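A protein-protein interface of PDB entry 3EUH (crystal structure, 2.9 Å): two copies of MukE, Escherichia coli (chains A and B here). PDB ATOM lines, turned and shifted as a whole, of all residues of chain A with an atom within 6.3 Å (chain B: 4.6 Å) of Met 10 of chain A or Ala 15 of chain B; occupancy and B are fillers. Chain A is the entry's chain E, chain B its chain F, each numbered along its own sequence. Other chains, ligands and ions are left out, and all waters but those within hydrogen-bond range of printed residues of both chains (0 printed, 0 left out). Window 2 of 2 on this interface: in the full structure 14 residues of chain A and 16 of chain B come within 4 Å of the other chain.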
ATOM      1  N   VAL A   9       2.007  12.443 -29.077  1.00  0.00           N
ATOM      2  CA  VAL A   9       3.097  13.013 -29.937  1.00  0.00           C
ATOM      3  C   VAL A   9       4.478  12.700 -29.383  1.00  0.00           C
ATOM      4  O   VAL A   9       5.272  11.991 -30.002  1.00  0.00           O
ATOM      5  CB  VAL A   9       2.991  14.550 -30.049  1.00  0.00           C
ATOM      6  CG1 VAL A   9       4.193  15.109 -30.797  1.00  0.00           C
ATOM      7  CG2 VAL A   9       1.712  14.922 -30.759  1.00  0.00           C
ATOM      8  N   MET A  10       4.748  13.251 -28.209  1.00  0.00           N
ATOM      9  CA  MET A  10       6.023  13.076 -27.533  1.00  0.00           C
ATOM     10  C   MET A  10       5.806  12.294 -26.234  1.00  0.00           C
ATOM     11  O   MET A  10       4.729  12.351 -25.641  1.00  0.00           O
ATOM     12  CB  MET A  10       6.606  14.465 -27.235  1.00  0.00           C
ATOM     13  CG  MET A  10       7.924  14.493 -26.477  1.00  0.00           C
ATOM     14  SD  MET A  10       8.424  16.188 -26.083  1.00  0.00           S
ATOM     15  CE  MET A  10       9.171  16.688 -27.655  1.00  0.00           C
ATOM     16  N   PRO A  11       6.811  11.523 -25.794  1.00  0.00           N
ATOM     17  CA  PRO A  11       6.607  10.787 -24.544  1.00  0.00           C
ATOM     18  C   PRO A  11       6.419  11.786 -23.403  1.00  0.00           C
ATOM     19  O   PRO A  11       7.236  12.689 -23.210  1.00  0.00           O
ATOM     20  CB  PRO A  11       7.892   9.982 -24.408  1.00  0.00           C
ATOM     21  CG  PRO A  11       8.246   9.702 -25.835  1.00  0.00           C
ATOM     22  CD  PRO A  11       8.007  11.038 -26.504  1.00  0.00           C
ATOM     23  N   VAL A  12       5.326  11.628 -22.668  1.00  0.00           N
ATOM     24  CA  VAL A  12       4.988  12.499 -21.544  1.00  0.00           C
ATOM     25  C   VAL A  12       6.185  13.018 -20.728  1.00  0.00           C
ATOM     26  O   VAL A  12       6.393  14.234 -20.605  1.00  0.00           O
ATOM     27  CB  VAL A  12       4.028  11.767 -20.588  1.00  0.00           C
ATOM     28  CG1 VAL A  12       3.530  12.717 -19.501  1.00  0.00           C
ATOM     29  CG2 VAL A  12       2.874  11.187 -21.385  1.00  0.00           C
ATOM     30  N   LYS A  13       6.962  12.096 -20.164  1.00  0.00           N
ATOM     31  CA  LYS A  13       8.111  12.476 -19.361  1.00  0.00           C
ATOM     32  C   LYS A  13       9.239  13.154 -20.126  1.00  0.00           C
ATOM     33  O   LYS A  13      10.108  13.764 -19.514  1.00  0.00           O
ATOM     34  CB  LYS A  13       8.661  11.272 -18.603  1.00  0.00           C
ATOM     35  CG  LYS A  13       7.952  11.004 -17.301  1.00  0.00           C
ATOM     36  CD  LYS A  13       8.684   9.938 -16.520  1.00  0.00           C
ATOM     37  CE  LYS A  13       7.983   9.601 -15.212  1.00  0.00           C
ATOM     38  NZ  LYS A  13       8.612   8.425 -14.526  1.00  0.00           N
ATOM     39  N   LEU A  14       9.253  13.053 -21.449  1.00  0.00           N
ATOM     40  CA  LEU A  14      10.307  13.726 -22.193  1.00  0.00           C
ATOM     41  C   LEU A  14       9.982  15.210 -22.059  1.00  0.00           C
ATOM     42  O   LEU A  14      10.855  16.031 -21.784  1.00  0.00           O
ATOM     43  CB  LEU A  14      10.294  13.327 -23.668  1.00  0.00           C
ATOM     44  CG  LEU A  14      11.637  13.398 -24.408  1.00  0.00           C
ATOM     45  CD1 LEU A  14      11.364  13.629 -25.881  1.00  0.00           C
ATOM     46  CD2 LEU A  14      12.506  14.522 -23.874  1.00  0.00           C
ATOM     47  N   ALA A  15       8.705  15.538 -22.231  1.00  0.00           N
ATOM     48  CA  ALA A  15       8.240  16.917 -22.134  1.00  0.00           C
ATOM     49  C   ALA A  15       8.364  17.500 -20.712  1.00  0.00           C
ATOM     50  O   ALA A  15       8.808  18.635 -20.535  1.00  0.00           O
ATOM     51  CB  ALA A  15       6.798  17.000 -22.621  1.00  0.00           C
ATOM     52  N   LEU A  18      12.178  18.485 -20.594  1.00  0.00           N
ATOM     53  CA  LEU A  18      12.509  19.589 -21.483  1.00  0.00           C
ATOM     54  C   LEU A  18      11.871  20.910 -21.072  1.00  0.00           C
ATOM     55  O   LEU A  18      12.328  21.963 -21.473  1.00  0.00           O
ATOM     56  CB  LEU A  18      12.095  19.250 -22.917  1.00  0.00           C
ATOM     57  CG  LEU A  18      13.214  18.970 -23.931  1.00  0.00           C
ATOM     58  CD1 LEU A  18      14.133  17.868 -23.429  1.00  0.00           C
ATOM     59  CD2 LEU A  18      12.596  18.572 -25.259  1.00  0.00           C
ATOM     60  N   ARG A  60      19.615  11.906 -30.165  1.00  0.00           N
ATOM     61  CA  ARG A  60      19.190  12.532 -31.403  1.00  0.00           C
ATOM     62  C   ARG A  60      20.216  13.460 -32.025  1.00  0.00           C
ATOM     63  O   ARG A  60      19.972  14.005 -33.102  1.00  0.00           O
ATOM     64  CB  ARG A  60      17.891  13.294 -31.164  1.00  0.00           C
ATOM     65  CG  ARG A  60      16.769  12.476 -30.495  1.00  0.00           C
ATOM     66  CD  ARG A  60      15.491  13.285 -30.554  1.00  0.00           C
ATOM     67  NE  ARG A  60      15.578  14.211 -31.686  1.00  0.00           N
ATOM     68  CZ  ARG A  60      14.593  15.000 -32.097  1.00  0.00           C
ATOM     69  NH1 ARG A  60      13.422  14.975 -31.469  1.00  0.00           N
ATOM     70  NH2 ARG A  60      14.788  15.819 -33.128  1.00  0.00           N
ATOM     71  N   MET B  10       3.395  21.750 -21.964  1.00  0.00           N
ATOM     72  CA  MET B  10       4.286  22.261 -22.991  1.00  0.00           C
ATOM     73  C   MET B  10       3.540  22.278 -24.319  1.00  0.00           C
ATOM     74  O   MET B  10       3.132  21.229 -24.824  1.00  0.00           O
ATOM     75  CB  MET B  10       5.526  21.380 -23.133  1.00  0.00           C
ATOM     76  CG  MET B  10       6.484  21.909 -24.191  1.00  0.00           C
ATOM     77  SD  MET B  10       7.546  20.671 -24.922  1.00  0.00           S
ATOM     78  CE  MET B  10       8.776  20.483 -23.616  1.00  0.00           C
ATOM     79  N   PRO B  11       3.351  23.472 -24.902  1.00  0.00           N
ATOM     80  CA  PRO B  11       2.652  23.636 -26.179  1.00  0.00           C
ATOM     81  C   PRO B  11       2.861  22.466 -27.134  1.00  0.00           C
ATOM     82  O   PRO B  11       3.987  22.150 -27.513  1.00  0.00           O
ATOM     83  CB  PRO B  11       3.232  24.937 -26.709  1.00  0.00           C
ATOM     84  CG  PRO B  11       3.328  25.750 -25.453  1.00  0.00           C
ATOM     85  CD  PRO B  11       3.899  24.759 -24.438  1.00  0.00           C
ATOM     86  N   VAL B  12       1.757  21.829 -27.510  1.00  0.00           N
ATOM     87  CA  VAL B  12       1.769  20.681 -28.412  1.00  0.00           C
ATOM     88  C   VAL B  12       2.555  20.863 -29.712  1.00  0.00           C
ATOM     89  O   VAL B  12       3.363  20.011 -30.081  1.00  0.00           O
ATOM     90  CB  VAL B  12       0.326  20.269 -28.769  1.00  0.00           C
ATOM     91  CG1 VAL B  12       0.329  19.244 -29.898  1.00  0.00           C
ATOM     92  CG2 VAL B  12      -0.362  19.700 -27.533  1.00  0.00           C
ATOM     93  N   LYS B  13       2.314  21.961 -30.413  1.00  0.00           N
ATOM     94  CA  LYS B  13       3.013  22.201 -31.663  1.00  0.00           C
ATOM     95  C   LYS B  13       4.500  22.489 -31.445  1.00  0.00           C
ATOM     96  O   LYS B  13       5.268  22.583 -32.405  1.00  0.00           O
ATOM     97  CB  LYS B  13       2.328  23.340 -32.409  1.00  0.00           C
ATOM     98  CG  LYS B  13       0.843  23.066 -32.631  1.00  0.00           C
ATOM     99  CD  LYS B  13       0.082  24.306 -33.076  1.00  0.00           C
ATOM    100  CE  LYS B  13      -1.428  24.087 -33.022  1.00  0.00           C
ATOM    101  NZ  LYS B  13      -2.183  25.343 -33.315  1.00  0.00           N
ATOM    102  N   LEU B  14       4.905  22.623 -30.182  1.00  0.00           N
ATOM    103  CA  LEU B  14       6.308  22.866 -29.847  1.00  0.00           C
ATOM    104  C   LEU B  14       7.031  21.532 -29.860  1.00  0.00           C
ATOM    105  O   LEU B  14       8.146  21.423 -30.358  1.00  0.00           O
ATOM    106  CB  LEU B  14       6.444  23.496 -28.458  1.00  0.00           C
ATOM    107  CG  LEU B  14       7.878  23.573 -27.916  1.00  0.00           C
ATOM    108  CD1 LEU B  14       8.720  24.474 -28.803  1.00  0.00           C
ATOM    109  CD2 LEU B  14       7.868  24.089 -26.486  1.00  0.00           C
ATOM    110  N   ALA B  15       6.395  20.520 -29.286  1.00  0.00           N
ATOM    111  CA  ALA B  15       6.968  19.186 -29.267  1.00  0.00           C
ATOM    112  C   ALA B  15       7.072  18.733 -30.720  1.00  0.00           C
ATOM    113  O   ALA B  15       8.034  18.082 -31.116  1.00  0.00           O
ATOM    114  CB  ALA B  15       6.071  18.242 -28.484  1.00  0.00           C
ATOM    115  N   GLN B  16       6.067  19.092 -31.510  1.00  0.00           N
ATOM    116  CA  GLN B  16       6.037  18.736 -32.918  1.00  0.00           C
ATOM    117  C   GLN B  16       7.220  19.351 -33.647  1.00  0.00           C
ATOM    118  O   GLN B  16       7.680  18.827 -34.659  1.00  0.00           O
ATOM    119  CB  GLN B  16       4.734  19.213 -33.566  1.00  0.00           C
ATOM    120  CG  GLN B  16       3.504  18.393 -33.198  1.00  0.00           C
ATOM    121  CD  GLN B  16       2.310  18.739 -34.071  1.00  0.00           C
ATOM    122  OE1 GLN B  16       2.388  18.668 -35.300  1.00  0.00           O
ATOM    123  NE2 GLN B  16       1.200  19.118 -33.442  1.00  0.00           N
ATOM    124  N   ALA B  17       7.702  20.478 -33.142  1.00  0.00           N
ATOM    125  CA  ALA B  17       8.848  21.129 -33.754  1.00  0.00           C
ATOM    126  C   ALA B  17      10.075  20.384 -33.257  1.00  0.00           C
ATOM    127  O   ALA B  17      10.972  20.042 -34.028  1.00  0.00           O
ATOM    128  CB  ALA B  17       8.908  22.587 -33.335  1.00  0.00           C
ATOM    129  N   LEU B  18      10.082  20.123 -31.953  1.00  0.00           N
ATOM    130  CA  LEU B  18      11.172  19.422 -31.284  1.00  0.00           C
ATOM    131  C   LEU B  18      11.441  18.023 -31.829  1.00  0.00           C
ATOM    132  O   LEU B  18      12.602  17.643 -32.016  1.00  0.00           O
ATOM    133  CB  LEU B  18      10.880  19.332 -29.781  1.00  0.00           C
ATOM    134  CG  LEU B  18      11.465  20.376 -28.823  1.00  0.00           C
ATOM    135  CD1 LEU B  18      11.738  21.688 -29.534  1.00  0.00           C
ATOM    136  CD2 LEU B  18      10.500  20.562 -27.661  1.00  0.00           C
ATOM    137  N   ALA B  19      10.370  17.267 -32.081  1.00  0.00           N
ATOM    138  CA  ALA B  19      10.469  15.897 -32.583  1.00  0.00           C
ATOM    139  C   ALA B  19      10.908  15.801 -34.043  1.00  0.00           C
ATOM    140  O   ALA B  19      11.492  14.796 -34.451  1.00  0.00           O
ATOM    141  CB  ALA B  19       9.144  15.178 -32.388  1.00  0.00           C
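The guanidinium group of Arg 60 of chain A is in hydrogen-bond range of the backbone carbonyl oxygen of Leu 18 of chain B (2.8 Å).
Met 10 of chain A touches Ala 15 of chain B, and with the chains exchanged Ala 15 of chain A touches Met 10 of chain B.
Met 10 of chain A touches Leu 18 of chain B, and with the chains exchanged Leu 18 of chain A touches Met 10 of chain B.
Leu 18 of chain B touches its own counterpart, Leu 18 of chain A.
Positions printed for both chains: 10, 11, 12, 13, 14, 15 and 18.
Among the printed residues, merely in contact across the chains: Arg 60 of chain A with Ala 19 of chain B (3.3 Å), Met 10 of chain A with Ala 15 of chain B (3.6 Å), Ala 15 of chain A with Met 10 of chain B (3.6 Å), Leu 18 of chain A with Met 10 of chain B (3.6 Å), Leu 18 of chain A with Leu 18 of chain B (3.8 Å) and Met 10 of chain A with Leu 18 of chain B (3.8 Å).
Met 10 of chain A touches just these residues of chain B: Ala 15 (3.6 Å) and Leu 18 (3.8 Å).
Ala 15 of chain B touches one residue of chain A.
Of the printed residues of chain B, Leu 18 of chain A touches Met 10 (3.6 Å) and Leu 18 (3.8 Å).
Of the printed residues of chain A, Leu 18 of chain B touches Met 10 (3.8 Å), Leu 18 (3.8 Å) and Arg 60 (2.8 Å).
Printed residues of chain A within 4 Å of Ala 19 of chain B: Arg 60 (3.3 Å).
Of the printed residues of chain B, Arg 60 of chain A touches Leu 18 and Ala 19.
Of the printed residues of chain B, Ala 15 of chain A touches Met 10.
Ala 17 of chain B touches none of the printed residues of chain A.
The nearest printed residue of chain B that does not touch Met 10 of chain A is Ala 19 of chain B (4.6 Å).
The nearest printed residue of chain A that does not touch Met 10 of chain B is Met 10 of chain A (4.7 Å).
Of the 9 printed residues of chain A, 4 touch a printed residue of chain B.
Printed residues of chain A that touch a printed residue of chain B: Met 10, Ala 15, Leu 18 and Arg 60.
Hydrophobic or aromatic side chains of chain A within 4 Å of the printed part of chain B: Met 10 and Leu 18.
Hydrophobic or aromatic side chains of chain B within 4 Å of the printed part of chain A: Met 10, Ala 15 and Leu 18.
Along chain B the printed residues that touch a printed residue of chain A span positions 10 to 19.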
